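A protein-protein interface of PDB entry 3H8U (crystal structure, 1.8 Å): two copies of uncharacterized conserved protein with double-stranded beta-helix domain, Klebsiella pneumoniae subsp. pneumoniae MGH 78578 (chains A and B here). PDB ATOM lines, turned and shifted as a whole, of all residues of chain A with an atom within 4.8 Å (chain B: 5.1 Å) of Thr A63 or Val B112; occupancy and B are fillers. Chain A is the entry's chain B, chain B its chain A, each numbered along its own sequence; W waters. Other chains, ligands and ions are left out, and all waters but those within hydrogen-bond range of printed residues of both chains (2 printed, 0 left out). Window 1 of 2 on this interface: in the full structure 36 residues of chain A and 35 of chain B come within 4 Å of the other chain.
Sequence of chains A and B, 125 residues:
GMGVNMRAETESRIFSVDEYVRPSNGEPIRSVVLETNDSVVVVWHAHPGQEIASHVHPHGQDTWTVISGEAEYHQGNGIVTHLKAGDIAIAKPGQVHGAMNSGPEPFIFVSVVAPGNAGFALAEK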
ATOM      1  N   GLN A  61     -11.813  19.352   4.145  1.00  0.00           N
ATOM      2  CA  GLN A  61     -13.082  19.180   3.510  1.00  0.00           C
ATOM      3  C   GLN A  61     -12.956  18.154   2.405  1.00  0.00           C
ATOM      4  O   GLN A  61     -11.971  18.137   1.676  1.00  0.00           O
ATOM      5  CB  GLN A  61     -13.568  20.514   2.939  1.00  0.00           C
ATOM      6  CG  GLN A  61     -14.903  20.441   2.219  1.00  0.00           C
ATOM      7  CD  GLN A  61     -15.462  21.820   1.908  1.00  0.00           C
ATOM      8  OE1 GLN A  61     -15.337  22.762   2.714  1.00  0.00           O
ATOM      9  NE2 GLN A  61     -16.099  21.948   0.749  1.00  0.00           N
ATOM     10  N   ASP A  62     -13.993  17.348   2.257  1.00  0.00           N
ATOM     11  CA  ASP A  62     -14.094  16.391   1.170  1.00  0.00           C
ATOM     12  C   ASP A  62     -15.363  16.694   0.372  1.00  0.00           C
ATOM     13  O   ASP A  62     -16.495  16.573   0.897  1.00  0.00           O
ATOM     14  CB  ASP A  62     -14.083  14.966   1.710  1.00  0.00           C
ATOM     15  CG  ASP A  62     -13.975  13.928   0.643  1.00  0.00           C
ATOM     16  OD1 ASP A  62     -13.881  14.270  -0.562  1.00  0.00           O
ATOM     17  OD2 ASP A  62     -13.959  12.746   1.029  1.00  0.00           O
ATOM     18  N   THR A  63     -15.165  17.119  -0.876  1.00  0.00           N
ATOM     19  CA  THR A  63     -16.254  17.483  -1.792  1.00  0.00           C
ATOM     20  C   THR A  63     -16.350  16.399  -2.864  1.00  0.00           C
ATOM     21  O   THR A  63     -15.407  16.181  -3.635  1.00  0.00           O
ATOM     22  CB  THR A  63     -15.981  18.835  -2.487  1.00  0.00           C
ATOM     23  OG1 THR A  63     -15.864  19.836  -1.496  1.00  0.00           O
ATOM     24  CG2 THR A  63     -17.106  19.240  -3.425  1.00  0.00           C
ATOM     25  N   TRP A  64     -17.471  15.697  -2.866  1.00  0.00           N
ATOM     26  CA  TRP A  64     -17.744  14.650  -3.861  1.00  0.00           C
ATOM     27  C   TRP A  64     -18.645  15.192  -4.959  1.00  0.00           C
ATOM     28  O   TRP A  64     -19.670  15.864  -4.694  1.00  0.00           O
ATOM     29  CB  TRP A  64     -18.492  13.504  -3.207  1.00  0.00           C
ATOM     30  CG  TRP A  64     -17.751  12.717  -2.172  1.00  0.00           C
ATOM     31  CD1 TRP A  64     -16.498  12.965  -1.624  1.00  0.00           C
ATOM     32  CD2 TRP A  64     -18.228  11.534  -1.548  1.00  0.00           C
ATOM     33  NE1 TRP A  64     -16.179  11.975  -0.737  1.00  0.00           N
ATOM     34  CE2 TRP A  64     -17.230  11.095  -0.656  1.00  0.00           C
ATOM     35  CE3 TRP A  64     -19.409  10.775  -1.679  1.00  0.00           C
ATOM     36  CZ2 TRP A  64     -17.366   9.935   0.096  1.00  0.00           C
ATOM     37  CZ3 TRP A  64     -19.536   9.633  -0.910  1.00  0.00           C
ATOM     38  CH2 TRP A  64     -18.535   9.231  -0.043  1.00  0.00           C
ATOM     39  N   THR A  65     -18.293  14.887  -6.202  1.00  0.00           N
ATOM     40  CA  THR A  65     -19.172  15.131  -7.314  1.00  0.00           C
ATOM     41  C   THR A  65     -19.478  13.802  -7.963  1.00  0.00           C
ATOM     42  O   THR A  65     -18.575  13.113  -8.452  1.00  0.00           O
ATOM     43  CB  THR A  65     -18.536  16.118  -8.345  1.00  0.00           C
ATOM     44  OG1 THR A  65     -18.300  17.379  -7.705  1.00  0.00           O
ATOM     45  CG2 THR A  65     -19.470  16.340  -9.510  1.00  0.00           C
ATOM     46  N   ILE A  88     -23.655  16.881  -5.508  1.00  0.00           N
ATOM     47  CA  ILE A  88     -22.429  17.202  -4.780  1.00  0.00           C
ATOM     48  C   ILE A  88     -22.685  16.871  -3.311  1.00  0.00           C
ATOM     49  O   ILE A  88     -23.727  17.223  -2.756  1.00  0.00           O
ATOM     50  CB  ILE A  88     -22.085  18.720  -4.881  1.00  0.00           C
ATOM     51  CG1 ILE A  88     -21.816  19.131  -6.347  1.00  0.00           C
ATOM     52  CG2 ILE A  88     -20.949  19.090  -3.971  1.00  0.00           C
ATOM     53  CD1 ILE A  88     -22.021  20.609  -6.589  1.00  0.00           C
ATOM     54  N   ALA A  89     -21.738  16.153  -2.718  1.00  0.00           N
ATOM     55  CA  ALA A  89     -21.834  15.800  -1.302  1.00  0.00           C
ATOM     56  C   ALA A  89     -20.605  16.404  -0.597  1.00  0.00           C
ATOM     57  O   ALA A  89     -19.472  16.182  -1.002  1.00  0.00           O
ATOM     58  CB  ALA A  89     -21.865  14.275  -1.152  1.00  0.00           C
ATOM     59  N   ILE A  90     -20.831  17.149   0.469  1.00  0.00           N
ATOM     60  CA  ILE A  90     -19.729  17.818   1.170  1.00  0.00           C
ATOM     61  C   ILE A  90     -19.619  17.338   2.600  1.00  0.00           C
ATOM     62  O   ILE A  90     -20.603  17.362   3.305  1.00  0.00           O
ATOM     63  CB  ILE A  90     -19.889  19.348   1.144  1.00  0.00           C
ATOM     64  CG1 ILE A  90     -19.821  19.823  -0.315  1.00  0.00           C
ATOM     65  CG2 ILE A  90     -18.816  19.988   2.035  1.00  0.00           C
ATOM     66  CD1 ILE A  90     -19.924  21.317  -0.537  1.00  0.00           C
ATOM     67  N   VAL A 110     -16.080  11.708  -8.017  1.00  0.00           N
ATOM     68  CA  VAL A 110     -14.808  12.384  -7.831  1.00  0.00           C
ATOM     69  C   VAL A 110     -14.787  13.055  -6.472  1.00  0.00           C
ATOM     70  O   VAL A 110     -15.690  13.824  -6.151  1.00  0.00           O
ATOM     71  CB  VAL A 110     -14.573  13.447  -8.908  1.00  0.00           C
ATOM     72  CG1 VAL A 110     -13.233  14.174  -8.647  1.00  0.00           C
ATOM     73  CG2 VAL A 110     -14.605  12.827 -10.287  1.00  0.00           C
ATOM     74  N   SER A 111     -13.748  12.772  -5.688  1.00  0.00           N
ATOM     75  CA  SER A 111     -13.554  13.362  -4.362  1.00  0.00           C
ATOM     76  C   SER A 111     -12.407  14.359  -4.427  1.00  0.00           C
ATOM     77  O   SER A 111     -11.368  14.054  -4.965  1.00  0.00           O
ATOM     78  CB  SER A 111     -13.215  12.277  -3.328  1.00  0.00           C
ATOM     79  OG  SER A 111     -12.544  12.839  -2.200  1.00  0.00           O
ATOM     80  N   VAL A 112     -12.643  15.573  -3.951  1.00  0.00           N
ATOM     81  CA  VAL A 112     -11.597  16.578  -3.793  1.00  0.00           C
ATOM     82  C   VAL A 112     -11.499  16.889  -2.283  1.00  0.00           C
ATOM     83  O   VAL A 112     -12.388  17.514  -1.661  1.00  0.00           O
ATOM     84  CB  VAL A 112     -11.860  17.871  -4.619  1.00  0.00           C
ATOM     85  CG1 VAL A 112     -10.725  18.903  -4.433  1.00  0.00           C
ATOM     86  CG2 VAL A 112     -12.067  17.542  -6.087  1.00  0.00           C
ATOM     87  N   SER B  39     -12.393  25.257   0.944  1.00  0.00           N
ATOM     88  CA  SER B  39     -12.714  25.248  -0.489  1.00  0.00           C
ATOM     89  C   SER B  39     -13.888  26.177  -0.790  1.00  0.00           C
ATOM     90  O   SER B  39     -14.729  26.468   0.063  1.00  0.00           O
ATOM     91  CB  SER B  39     -13.145  23.854  -0.984  1.00  0.00           C
ATOM     92  OG  SER B  39     -12.112  22.869  -0.804  1.00  0.00           O
ATOM     93  N   VAL B  40     -13.944  26.576  -2.047  1.00  0.00           N
ATOM     94  CA  VAL B  40     -15.131  27.199  -2.615  1.00  0.00           C
ATOM     95  C   VAL B  40     -15.617  26.280  -3.748  1.00  0.00           C
ATOM     96  O   VAL B  40     -14.836  25.903  -4.625  1.00  0.00           O
ATOM     97  CB  VAL B  40     -14.819  28.626  -3.113  1.00  0.00           C
ATOM     98  CG1 VAL B  40     -15.996  29.207  -3.880  1.00  0.00           C
ATOM     99  CG2 VAL B  40     -14.459  29.547  -1.946  1.00  0.00           C
ATOM    100  N   VAL B  41     -16.886  25.899  -3.698  1.00  0.00           N
ATOM    101  CA  VAL B  41     -17.470  24.959  -4.631  1.00  0.00           C
ATOM    102  C   VAL B  41     -18.489  25.758  -5.436  1.00  0.00           C
ATOM    103  O   VAL B  41     -19.397  26.411  -4.838  1.00  0.00           O
ATOM    104  CB  VAL B  41     -18.173  23.786  -3.879  1.00  0.00           C
ATOM    105  CG1 VAL B  41     -18.877  22.834  -4.864  1.00  0.00           C
ATOM    106  CG2 VAL B  41     -17.182  23.021  -3.005  1.00  0.00           C
ATOM    107  N   GLN B  61      -5.460  25.720  -6.075  1.00  0.00           N
ATOM    108  CA  GLN B  61      -5.744  24.727  -7.094  1.00  0.00           C
ATOM    109  C   GLN B  61      -7.227  24.765  -7.429  1.00  0.00           C
ATOM    110  O   GLN B  61      -8.083  24.877  -6.526  1.00  0.00           O
ATOM    111  CB  GLN B  61      -5.362  23.332  -6.589  1.00  0.00           C
ATOM    112  CG  GLN B  61      -5.706  22.218  -7.575  1.00  0.00           C
ATOM    113  CD  GLN B  61      -5.200  20.917  -7.120  1.00  0.00           C
ATOM    114  OE1 GLN B  61      -4.078  20.838  -6.560  1.00  0.00           O
ATOM    115  NE2 GLN B  61      -5.939  19.849  -7.432  1.00  0.00           N
ATOM    116  N   ASP B  62      -7.531  24.691  -8.724  1.00  0.00           N
ATOM    117  CA  ASP B  62      -8.889  24.636  -9.205  1.00  0.00           C
ATOM    118  C   ASP B  62      -9.114  23.302  -9.922  1.00  0.00           C
ATOM    119  O   ASP B  62      -8.525  23.020 -10.973  1.00  0.00           O
ATOM    120  CB  ASP B  62      -9.163  25.802 -10.152  1.00  0.00           C
ATOM    121  CG  ASP B  62     -10.636  25.961 -10.497  1.00  0.00           C
ATOM    122  OD1 ASP B  62     -11.491  25.169 -10.000  1.00  0.00           O
ATOM    123  OD2 ASP B  62     -10.926  26.916 -11.282  1.00  0.00           O
ATOM    124  N   THR B  63      -9.946  22.482  -9.311  1.00  0.00           N
ATOM    125  CA  THR B  63     -10.278  21.165  -9.821  1.00  0.00           C
ATOM    126  C   THR B  63     -11.702  21.204 -10.379  1.00  0.00           C
ATOM    127  O   THR B  63     -12.657  21.496  -9.645  1.00  0.00           O
ATOM    128  CB  THR B  63     -10.179  20.066  -8.719  1.00  0.00           C
ATOM    129  OG1 THR B  63      -8.863  20.084  -8.149  1.00  0.00           O
ATOM    130  CG2 THR B  63     -10.420  18.687  -9.359  1.00  0.00           C
ATOM    131  N   TRP B  64     -11.833  20.923 -11.679  1.00  0.00           N
ATOM    132  CA  TRP B  64     -13.124  20.867 -12.323  1.00  0.00           C
ATOM    133  C   TRP B  64     -13.569  19.450 -12.585  1.00  0.00           C
ATOM    134  O   TRP B  64     -12.807  18.631 -13.082  1.00  0.00           O
ATOM    135  CB  TRP B  64     -13.114  21.559 -13.687  1.00  0.00           C
ATOM    136  CG  TRP B  64     -12.777  22.992 -13.737  1.00  0.00           C
ATOM    137  CD1 TRP B  64     -12.491  23.825 -12.702  1.00  0.00           C
ATOM    138  CD2 TRP B  64     -12.755  23.800 -14.920  1.00  0.00           C
ATOM    139  NE1 TRP B  64     -12.294  25.094 -13.168  1.00  0.00           N
ATOM    140  CE2 TRP B  64     -12.430  25.107 -14.525  1.00  0.00           C
ATOM    141  CE3 TRP B  64     -12.996  23.540 -16.280  1.00  0.00           C
ATOM    142  CZ2 TRP B  64     -12.332  26.162 -15.424  1.00  0.00           C
ATOM    143  CZ3 TRP B  64     -12.899  24.592 -17.183  1.00  0.00           C
ATOM    144  CH2 TRP B  64     -12.573  25.887 -16.756  1.00  0.00           C
ATOM    145  N   VAL B 110     -18.440  21.315 -12.047  1.00  0.00           N
ATOM    146  CA  VAL B 110     -18.311  21.672 -10.663  1.00  0.00           C
ATOM    147  C   VAL B 110     -16.843  22.009 -10.477  1.00  0.00           C
ATOM    148  O   VAL B 110     -15.969  21.169 -10.690  1.00  0.00           O
ATOM    149  CB  VAL B 110     -18.707  20.516  -9.749  1.00  0.00           C
ATOM    150  CG1 VAL B 110     -18.374  20.875  -8.246  1.00  0.00           C
ATOM    151  CG2 VAL B 110     -20.181  20.173  -9.944  1.00  0.00           C
ATOM    152  N   SER B 111     -16.606  23.237 -10.037  1.00  0.00           N
ATOM    153  CA  SER B 111     -15.288  23.723  -9.667  1.00  0.00           C
ATOM    154  C   SER B 111     -15.073  23.718  -8.146  1.00  0.00           C
ATOM    155  O   SER B 111     -15.894  24.284  -7.403  1.00  0.00           O
ATOM    156  CB  SER B 111     -15.121  25.160 -10.168  1.00  0.00           C
ATOM    157  OG  SER B 111     -14.032  25.799  -9.532  1.00  0.00           O
ATOM    158  N   VAL B 112     -13.958  23.115  -7.719  1.00  0.00           N
ATOM    159  CA  VAL B 112     -13.529  23.171  -6.333  1.00  0.00           C
ATOM    160  C   VAL B 112     -12.178  23.891  -6.293  1.00  0.00           C
ATOM    161  O   VAL B 112     -11.179  23.334  -6.733  1.00  0.00           O
ATOM    162  CB  VAL B 112     -13.423  21.773  -5.695  1.00  0.00           C
ATOM    163  CG1 VAL B 112     -13.018  21.889  -4.174  1.00  0.00           C
ATOM    164  CG2 VAL B 112     -14.738  20.999  -5.873  1.00  0.00           C
ATOM    165  N   VAL B 113     -12.189  25.120  -5.769  1.00  0.00           N
ATOM    166  CA  VAL B 113     -10.968  25.906  -5.575  1.00  0.00           C
ATOM    167  C   VAL B 113     -10.502  25.761  -4.140  1.00  0.00           C
ATOM    168  O   VAL B 113     -11.310  25.927  -3.217  1.00  0.00           O
ATOM    169  CB  VAL B 113     -11.220  27.384  -5.902  1.00  0.00           C
ATOM    170  CG1 VAL B 113     -10.034  28.261  -5.511  1.00  0.00           C
ATOM    171  CG2 VAL B 113     -11.503  27.522  -7.412  1.00  0.00           C
ATOM    172  N   ALA B 114      -9.224  25.437  -3.959  1.00  0.00           N
ATOM    173  CA  ALA B 114      -8.661  25.248  -2.623  1.00  0.00           C
ATOM    174  C   ALA B 114      -7.302  25.929  -2.542  1.00  0.00           C
ATOM    175  O   ALA B 114      -6.476  25.763  -3.453  1.00  0.00           O
ATOM    176  CB  ALA B 114      -8.521  23.757  -2.303  1.00  0.00           C
HETATM  177  O   HOH W   1     -16.910  24.748   0.162  1.00  0.00           O
HETATM  178  O   HOH W   2     -13.214  20.182  -0.773  1.00  0.00           O
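The side-chain hydroxyl (OG1) of Thr B63 lies within hydrogen-bond range of the side-chain amide nitrogen (NE2) of Gln B61 (3.0 Å).
The backbone NH (N) of Val B112 is in hydrogen-bond range of the backbone carbonyl oxygen (O) of Thr B63, 2.8 Å away.
OG1 of Thr A63 lies within hydrogen-bond range of NE2 of Gln A61.
The backbone carbonyl oxygen (O) of Thr A63 is in hydrogen-bond range of the backbone NH (N) of Val A112.
N of Thr A65 sits at hydrogen-bond distance from O of Val A110, 2.8 Å away.
Gln A61 touches Ser B39 (NE2 to CB, 3.9 Å).
OG1 of Thr A63 touches CG2 of Val B41 (3.8 Å).
Val B112 touches Thr A63 (CG2 to CG2, 3.8 Å).
OG1 of Thr A65 touches CG1 of Val B110, at 3.5 Å.
Val B110 touches Ile A88.
CG2 of Val A112 touches CG2 of Thr B63 (3.8 Å).
CG1 of Val A112 touches CG1 of Val B112, 3.8 Å away.
Thr A63 touches just these residues of chain B: Val B41 and Val B112.
Val B112 touches just these residues of chain A: Thr A63 (3.8 Å) and Val A112 (3.8 Å).
Printed residues of chain B within 4 Å of Gln A61: Ser B39.
Printed residues of chain B within 4 Å of Thr A65: Val B110 (3.5 Å).
Of the printed residues of chain B, Ile A88 touches Val B110.
The nearest residue of chain B that does not touch Thr A63 is Ser B39 (4.9 Å).
The nearest printed residue of chain A that does not touch Val B110 is Thr A63 (5.2 Å).
Of the 11 printed residues of chain A, 5 touch a printed residue of chain B.
Hydrophobic or aromatic side chains of chain A that line the printed part of chain B: Ile A88 and Val A112.
Among the printed residues, 7 pairs touch across the chains.
Among the printed residues, no Asp or Glu carboxylate lies within 4 Å of a Lys or Arg side-chain nitrogen of the other chain.
Thr A63 touches Val B112, and with the chains exchanged Val A112 touches Thr B63.
Val B112 touches its own counterpart, Val A112.
7 positions are printed for both chains.
Water W2 lies within hydrogen-bond range of the side-chain hydroxyl (OG1) of Thr A63 (2.8 Å), the side-chain hydroxyl (OG) of Ser B39 (2.9 Å), the backbone carbonyl oxygen (O) of Val A112 (2.9 Å) and the backbone carbonyl oxygen (O) of Gln A61 (3.4 Å).
Water W1 bridges O of Ser B39 (2.8 Å) and NE2 of Gln A61 (3.0 Å).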
